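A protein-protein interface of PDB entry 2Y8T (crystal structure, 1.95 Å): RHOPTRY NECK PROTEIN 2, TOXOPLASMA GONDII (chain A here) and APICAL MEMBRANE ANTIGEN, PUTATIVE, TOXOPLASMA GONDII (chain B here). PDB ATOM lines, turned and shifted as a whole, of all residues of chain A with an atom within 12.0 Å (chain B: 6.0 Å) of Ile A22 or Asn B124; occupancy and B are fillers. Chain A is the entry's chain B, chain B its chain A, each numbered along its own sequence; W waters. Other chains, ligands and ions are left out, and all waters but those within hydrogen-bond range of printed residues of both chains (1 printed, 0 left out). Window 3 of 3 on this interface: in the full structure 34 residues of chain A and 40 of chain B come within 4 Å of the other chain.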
ATOM      1  N   VAL A  18     -12.587   4.078  -9.243  1.00  0.00           N
ATOM      2  CA  VAL A  18     -13.105   3.865 -10.556  1.00  0.00           C
ATOM      3  C   VAL A  18     -14.548   3.362 -10.408  1.00  0.00           C
ATOM      4  O   VAL A  18     -14.853   2.785  -9.397  1.00  0.00           O
ATOM      5  CB  VAL A  18     -12.130   2.824 -11.089  1.00  0.00           C
ATOM      6  CG1 VAL A  18     -12.679   1.528 -11.475  1.00  0.00           C
ATOM      7  CG2 VAL A  18     -10.919   3.464 -11.794  1.00  0.00           C
ATOM      8  N   THR A  19     -15.453   3.657 -11.337  1.00  0.00           N
ATOM      9  CA  THR A  19     -16.757   2.963 -11.323  1.00  0.00           C
ATOM     10  C   THR A  19     -16.902   1.975 -12.475  1.00  0.00           C
ATOM     11  O   THR A  19     -16.650   2.325 -13.640  1.00  0.00           O
ATOM     12  CB  THR A  19     -17.972   3.888 -11.245  1.00  0.00           C
ATOM     13  OG1 THR A  19     -19.180   3.106 -11.086  1.00  0.00           O
ATOM     14  CG2 THR A  19     -18.095   4.878 -12.450  1.00  0.00           C
ATOM     15  N   ASN A  20     -17.311   0.765 -12.116  1.00  0.00           N
ATOM     16  CA  ASN A  20     -17.450  -0.355 -13.024  1.00  0.00           C
ATOM     17  C   ASN A  20     -18.941  -0.798 -12.984  1.00  0.00           C
ATOM     18  O   ASN A  20     -19.558  -0.852 -11.909  1.00  0.00           O
ATOM     19  CB  ASN A  20     -16.534  -1.476 -12.545  1.00  0.00           C
ATOM     20  CG  ASN A  20     -16.762  -2.773 -13.288  1.00  0.00           C
ATOM     21  OD1 ASN A  20     -17.570  -3.592 -12.837  1.00  0.00           O
ATOM     22  ND2 ASN A  20     -16.099  -2.953 -14.458  1.00  0.00           N
ATOM     23  N   GLU A  21     -19.516  -1.065 -14.154  1.00  0.00           N
ATOM     24  CA  GLU A  21     -20.932  -1.407 -14.246  1.00  0.00           C
ATOM     25  C   GLU A  21     -21.304  -2.712 -13.557  1.00  0.00           C
ATOM     26  O   GLU A  21     -22.461  -2.874 -13.203  1.00  0.00           O
ATOM     27  CB  GLU A  21     -21.413  -1.406 -15.705  1.00  0.00           C
ATOM     28  CG  GLU A  21     -21.397  -0.025 -16.354  1.00  0.00           C
ATOM     29  CD  GLU A  21     -21.935  -0.062 -17.773  1.00  0.00           C
ATOM     30  OE1 GLU A  21     -22.828  -0.911 -18.058  1.00  0.00           O
ATOM     31  OE2 GLU A  21     -21.492   0.781 -18.586  1.00  0.00           O
ATOM     32  N   ILE A  22     -20.353  -3.640 -13.353  1.00  0.00           N
ATOM     33  CA  ILE A  22     -20.652  -4.829 -12.571  1.00  0.00           C
ATOM     34  C   ILE A  22     -20.495  -4.654 -11.060  1.00  0.00           C
ATOM     35  O   ILE A  22     -21.320  -5.147 -10.281  1.00  0.00           O
ATOM     36  CB  ILE A  22     -19.863  -6.055 -12.979  1.00  0.00           C
ATOM     37  CG1 ILE A  22     -20.497  -6.729 -14.198  1.00  0.00           C
ATOM     38  CG2 ILE A  22     -19.964  -7.097 -11.851  1.00  0.00           C
ATOM     39  CD1 ILE A  22     -21.237  -5.813 -15.132  1.00  0.00           C
ATOM     40  N   LEU A  23     -19.421  -4.003 -10.638  1.00  0.00           N
ATOM     41  CA  LEU A  23     -19.120  -3.928  -9.219  1.00  0.00           C
ATOM     42  C   LEU A  23     -19.583  -2.668  -8.522  1.00  0.00           C
ATOM     43  O   LEU A  23     -19.519  -2.615  -7.318  1.00  0.00           O
ATOM     44  CB  LEU A  23     -17.605  -4.069  -9.021  1.00  0.00           C
ATOM     45  CG  LEU A  23     -16.995  -5.432  -9.402  1.00  0.00           C
ATOM     46  CD1 LEU A  23     -15.479  -5.419  -9.283  1.00  0.00           C
ATOM     47  CD2 LEU A  23     -17.560  -6.548  -8.568  1.00  0.00           C
ATOM     48  N   GLY A  24     -19.881  -1.622  -9.277  1.00  0.00           N
ATOM     49  CA  GLY A  24     -20.077  -0.289  -8.763  1.00  0.00           C
ATOM     50  C   GLY A  24     -18.743   0.357  -8.470  1.00  0.00           C
ATOM     51  O   GLY A  24     -17.714   0.080  -9.143  1.00  0.00           O
ATOM     52  N   VAL A  25     -18.753   1.243  -7.493  1.00  0.00           N
ATOM     53  CA  VAL A  25     -17.570   2.043  -7.182  1.00  0.00           C
ATOM     54  C   VAL A  25     -16.522   1.188  -6.512  1.00  0.00           C
ATOM     55  O   VAL A  25     -16.814   0.378  -5.633  1.00  0.00           O
ATOM     56  CB  VAL A  25     -17.923   3.279  -6.309  1.00  0.00           C
ATOM     57  CG1 VAL A  25     -16.604   4.031  -5.785  1.00  0.00           C
ATOM     58  CG2 VAL A  25     -18.830   4.201  -7.098  1.00  0.00           C
ATOM     59  N   THR A  26     -15.259   1.396  -6.879  1.00  0.00           N
ATOM     60  CA  THR A  26     -14.204   0.576  -6.366  1.00  0.00           C
ATOM     61  C   THR A  26     -13.033   1.576  -6.067  1.00  0.00           C
ATOM     62  O   THR A  26     -12.807   2.518  -6.832  1.00  0.00           O
ATOM     63  CB  THR A  26     -13.940  -0.421  -7.515  1.00  0.00           C
ATOM     64  OG1 THR A  26     -14.348  -1.782  -7.287  1.00  0.00           O
ATOM     65  CG2 THR A  26     -12.815  -0.157  -8.379  1.00  0.00           C
ATOM     66  N   CYS A  27     -12.356   1.417  -4.944  1.00  0.00           N
ATOM     67  CA  CYS A  27     -11.397   2.444  -4.496  1.00  0.00           C
ATOM     68  C   CYS A  27     -10.159   1.765  -3.980  1.00  0.00           C
ATOM     69  O   CYS A  27     -10.214   0.658  -3.592  1.00  0.00           O
ATOM     70  CB  CYS A  27     -12.010   3.321  -3.388  1.00  0.00           C
ATOM     71  SG  CYS A  27     -13.444   4.303  -3.918  1.00  0.00           S
ATOM     72  N   PHE B 116      -9.955  -9.969 -12.633  1.00  0.00           N
ATOM     73  CA  PHE B 116     -11.327 -10.369 -12.479  1.00  0.00           C
ATOM     74  C   PHE B 116     -11.584 -11.650 -13.275  1.00  0.00           C
ATOM     75  O   PHE B 116     -11.186 -11.759 -14.415  1.00  0.00           O
ATOM     76  CB  PHE B 116     -12.246  -9.280 -12.979  1.00  0.00           C
ATOM     77  CG  PHE B 116     -13.657  -9.436 -12.503  1.00  0.00           C
ATOM     78  CD1 PHE B 116     -14.001  -9.029 -11.195  1.00  0.00           C
ATOM     79  CD2 PHE B 116     -14.642  -9.997 -13.336  1.00  0.00           C
ATOM     80  CE1 PHE B 116     -15.321  -9.147 -10.707  1.00  0.00           C
ATOM     81  CE2 PHE B 116     -16.003 -10.126 -12.862  1.00  0.00           C
ATOM     82  CZ  PHE B 116     -16.335  -9.681 -11.562  1.00  0.00           C
ATOM     83  N   LEU B 120     -16.817 -15.332 -13.674  1.00  0.00           N
ATOM     84  CA  LEU B 120     -17.863 -14.404 -13.305  1.00  0.00           C
ATOM     85  C   LEU B 120     -18.394 -13.590 -14.480  1.00  0.00           C
ATOM     86  O   LEU B 120     -19.560 -13.207 -14.496  1.00  0.00           O
ATOM     87  CB  LEU B 120     -17.410 -13.489 -12.140  1.00  0.00           C
ATOM     88  CG  LEU B 120     -17.636 -13.945 -10.670  1.00  0.00           C
ATOM     89  CD1 LEU B 120     -17.571 -15.486 -10.424  1.00  0.00           C
ATOM     90  CD2 LEU B 120     -16.718 -13.205  -9.659  1.00  0.00           C
ATOM     91  N   LEU B 121     -17.571 -13.283 -15.473  1.00  0.00           N
ATOM     92  CA  LEU B 121     -18.100 -12.438 -16.541  1.00  0.00           C
ATOM     93  C   LEU B 121     -19.051 -13.215 -17.445  1.00  0.00           C
ATOM     94  O   LEU B 121     -19.991 -12.648 -18.015  1.00  0.00           O
ATOM     95  CB  LEU B 121     -16.957 -11.865 -17.387  1.00  0.00           C
ATOM     96  CG  LEU B 121     -16.056 -10.838 -16.675  1.00  0.00           C
ATOM     97  CD1 LEU B 121     -14.905 -10.511 -17.597  1.00  0.00           C
ATOM     98  CD2 LEU B 121     -16.869  -9.585 -16.318  1.00  0.00           C
ATOM     99  N   GLU B 122     -18.767 -14.495 -17.632  1.00  0.00           N
ATOM    100  CA  GLU B 122     -19.616 -15.300 -18.516  1.00  0.00           C
ATOM    101  C   GLU B 122     -20.995 -15.587 -17.932  1.00  0.00           C
ATOM    102  O   GLU B 122     -21.923 -15.873 -18.663  1.00  0.00           O
ATOM    103  CB  GLU B 122     -18.916 -16.559 -19.044  1.00  0.00           C
ATOM    104  CG  GLU B 122     -18.133 -17.375 -18.079  1.00  0.00           C
ATOM    105  CD  GLU B 122     -16.990 -18.121 -18.773  1.00  0.00           C
ATOM    106  OE1 GLU B 122     -16.725 -17.856 -19.980  1.00  0.00           O
ATOM    107  OE2 GLU B 122     -16.331 -18.959 -18.099  1.00  0.00           O
ATOM    108  N   LYS B 123     -21.186 -15.410 -16.635  1.00  0.00           N
ATOM    109  CA  LYS B 123     -22.564 -15.538 -16.128  1.00  0.00           C
ATOM    110  C   LYS B 123     -23.241 -14.260 -15.642  1.00  0.00           C
ATOM    111  O   LYS B 123     -24.160 -14.327 -14.826  1.00  0.00           O
ATOM    112  CB  LYS B 123     -22.706 -16.688 -15.121  1.00  0.00           C
ATOM    113  CG  LYS B 123     -21.605 -16.792 -14.102  1.00  0.00           C
ATOM    114  CD  LYS B 123     -21.570 -18.174 -13.489  1.00  0.00           C
ATOM    115  CE  LYS B 123     -20.304 -18.938 -13.870  1.00  0.00           C
ATOM    116  NZ  LYS B 123     -20.212 -19.258 -15.325  1.00  0.00           N
ATOM    117  N   ASN B 124     -22.822 -13.112 -16.179  1.00  0.00           N
ATOM    118  CA  ASN B 124     -23.382 -11.842 -15.795  1.00  0.00           C
ATOM    119  C   ASN B 124     -24.245 -11.192 -16.876  1.00  0.00           C
ATOM    120  O   ASN B 124     -23.811 -11.059 -18.016  1.00  0.00           O
ATOM    121  CB  ASN B 124     -22.265 -10.892 -15.355  1.00  0.00           C
ATOM    122  CG  ASN B 124     -22.794  -9.656 -14.712  1.00  0.00           C
ATOM    123  OD1 ASN B 124     -23.411  -8.825 -15.372  1.00  0.00           O
ATOM    124  ND2 ASN B 124     -22.555  -9.514 -13.419  1.00  0.00           N
ATOM    125  N   SER B 125     -25.447 -10.750 -16.503  1.00  0.00           N
ATOM    126  CA  SER B 125     -26.429 -10.253 -17.496  1.00  0.00           C
ATOM    127  C   SER B 125     -26.020  -8.926 -18.135  1.00  0.00           C
ATOM    128  O   SER B 125     -26.474  -8.573 -19.238  1.00  0.00           O
ATOM    129  CB  SER B 125     -27.857 -10.149 -16.908  1.00  0.00           C
ATOM    130  OG  SER B 125     -27.939  -9.160 -15.878  1.00  0.00           O
ATOM    131  N   ASN B 126     -25.193  -8.166 -17.441  1.00  0.00           N
ATOM    132  CA  ASN B 126     -24.757  -6.936 -18.018  1.00  0.00           C
ATOM    133  C   ASN B 126     -23.737  -7.174 -19.135  1.00  0.00           C
ATOM    134  O   ASN B 126     -23.676  -6.380 -20.052  1.00  0.00           O
ATOM    135  CB  ASN B 126     -24.259  -5.973 -16.933  1.00  0.00           C
ATOM    136  CG  ASN B 126     -23.754  -4.628 -17.503  1.00  0.00           C
ATOM    137  OD1 ASN B 126     -24.509  -3.656 -17.657  1.00  0.00           O
ATOM    138  ND2 ASN B 126     -22.465  -4.586 -17.826  1.00  0.00           N
ATOM    139  N   ILE B 127     -22.978  -8.263 -19.059  1.00  0.00           N
ATOM    140  CA  ILE B 127     -21.911  -8.562 -20.033  1.00  0.00           C
ATOM    141  C   ILE B 127     -22.427  -9.244 -21.311  1.00  0.00           C
ATOM    142  O   ILE B 127     -22.755 -10.441 -21.300  1.00  0.00           O
ATOM    143  CB  ILE B 127     -20.841  -9.456 -19.397  1.00  0.00           C
ATOM    144  CG1 ILE B 127     -20.215  -8.727 -18.189  1.00  0.00           C
ATOM    145  CG2 ILE B 127     -19.737  -9.867 -20.420  1.00  0.00           C
ATOM    146  CD1 ILE B 127     -19.512  -7.392 -18.523  1.00  0.00           C
ATOM    147  N   LYS B 128     -22.454  -8.499 -22.408  1.00  0.00           N
ATOM    148  CA  LYS B 128     -23.099  -8.980 -23.658  1.00  0.00           C
ATOM    149  C   LYS B 128     -22.201  -9.654 -24.723  1.00  0.00           C
ATOM    150  O   LYS B 128     -22.710 -10.362 -25.634  1.00  0.00           O
ATOM    151  CB  LYS B 128     -23.968  -7.879 -24.230  1.00  0.00           C
ATOM    152  CG  LYS B 128     -25.071  -7.544 -23.201  1.00  0.00           C
ATOM    153  CD  LYS B 128     -26.010  -6.460 -23.668  1.00  0.00           C
ATOM    154  CE  LYS B 128     -27.150  -6.254 -22.650  1.00  0.00           C
ATOM    155  NZ  LYS B 128     -28.256  -5.377 -23.225  1.00  0.00           N
ATOM    156  N   PHE B 139     -15.708  -5.527 -20.045  1.00  0.00           N
ATOM    157  CA  PHE B 139     -15.499  -5.189 -18.615  1.00  0.00           C
ATOM    158  C   PHE B 139     -14.620  -3.923 -18.511  1.00  0.00           C
ATOM    159  O   PHE B 139     -14.911  -2.993 -17.714  1.00  0.00           O
ATOM    160  CB  PHE B 139     -14.833  -6.389 -17.919  1.00  0.00           C
ATOM    161  CG  PHE B 139     -14.641  -6.240 -16.418  1.00  0.00           C
ATOM    162  CD1 PHE B 139     -15.740  -6.354 -15.521  1.00  0.00           C
ATOM    163  CD2 PHE B 139     -13.345  -6.065 -15.895  1.00  0.00           C
ATOM    164  CE1 PHE B 139     -15.529  -6.319 -14.094  1.00  0.00           C
ATOM    165  CE2 PHE B 139     -13.108  -5.985 -14.514  1.00  0.00           C
ATOM    166  CZ  PHE B 139     -14.233  -6.115 -13.590  1.00  0.00           C
ATOM    167  N   LYS B 142     -16.530  -0.761 -19.638  1.00  0.00           N
ATOM    168  CA  LYS B 142     -17.561  -0.501 -18.591  1.00  0.00           C
ATOM    169  C   LYS B 142     -16.929  -0.073 -17.287  1.00  0.00           C
ATOM    170  O   LYS B 142     -17.612  -0.091 -16.240  1.00  0.00           O
ATOM    171  CB  LYS B 142     -18.468  -1.751 -18.413  1.00  0.00           C
ATOM    172  CG  LYS B 142     -19.329  -1.947 -19.662  1.00  0.00           C
ATOM    173  CD  LYS B 142     -20.348  -3.111 -19.545  1.00  0.00           C
ATOM    174  CE  LYS B 142     -21.316  -3.031 -20.751  1.00  0.00           C
ATOM    175  NZ  LYS B 142     -22.144  -4.229 -20.676  1.00  0.00           N
HETATM  176  O   HOH W   1     -24.490  -0.912 -19.792  1.00  0.00           O
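The side-chain carboxylate (OE1) of Glu A21 lies close to the side-chain amide oxygen (OD1) of Asn B126 (3.2 Å). O of Phe B139 lies close to ND2 of Asn A20, 3.5 Å away. O of Lys B142 lies within hydrogen-bond range of N of Glu A21 (3.0 Å).
The side-chain amide oxygen (OD1) of Asn B124 sits at hydrogen-bond distance from the backbone NH (N) of Asn B126 (2.8 Å). The backbone carbonyl oxygen (O) of Asn B126 sits at hydrogen-bond distance from the side-chain amino group (NZ) of Lys B142 (2.7 Å). The backbone NH of Ile A22 lies within hydrogen-bond range of the side-chain amide oxygen of Asn A20, 2.8 Å away. The side-chain amide oxygen of Asn A20 lies within hydrogen-bond range of the backbone NH of Leu A23, at 2.9 Å.
Among the printed residues, pairs that only touch across the chains: Ile A22 with Asn B126 (3.2 Å), Asn A20 with Lys B142 (3.2 Å), Ile A22 with Asn B124 (3.5 Å), Thr A19 with Lys B142 (3.7 Å) and Leu A23 with Phe B116 (3.99 Å).
Leu B121 touches none of the printed residues of chain A. No residue of chain A comes within 4 Å of Lys B123. No residue of chain A comes within 4 Å of Ser B125. Of chain A, only Glu A21 and Ile A22 come within 4 Å of Asn B126. No residue of chain A comes within 4 Å of Ile B127. Printed residues of chain A within 4 Å of Phe B139: Asn A20. Of chain A, only Thr A19, Asn A20 and Glu A21 come within 4 Å of Lys B142. Printed residues of chain B within 4 Å of Thr A19: Lys B142. Printed residues of chain B within 4 Å of Asn A20: Phe B139 (3.4 Å) and Lys B142 (3.2 Å). Printed residues of chain B within 4 Å of Leu A23: Phe B116. Printed residues of chain B within 4 Å of Glu A21: Asn B126 (3.2 Å) and Lys B142 (3.0 Å). Val A18 touches none of the printed residues of chain B. Gly A24 touches none of the printed residues of chain B. The nearest residue of chain B that does not touch Ile A22 is Ile B127 (4.1 Å). The nearest printed residue of chain B that does not touch Asn A20 is Phe B116 (6.3 Å).
Of the 12 printed residues of chain B, 5 touch a printed residue of chain A. Hydrophobic or aromatic side chains of chain B within 4 Å of the printed part of chain A: Phe B116 and Phe B139. Hydrophobic or aromatic side chains of chain A within 4 Å of the printed part of chain B: Ile A22 and Leu A23. Among the printed residues, no Asp or Glu carboxylate lies within 4 Å of a Lys or Arg side-chain nitrogen of the other chain.
Water W1 bridges the side-chain carboxylate of Glu A21 (2.4 Å) and the side-chain amide oxygen of Asn B126 (3.5 Å).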
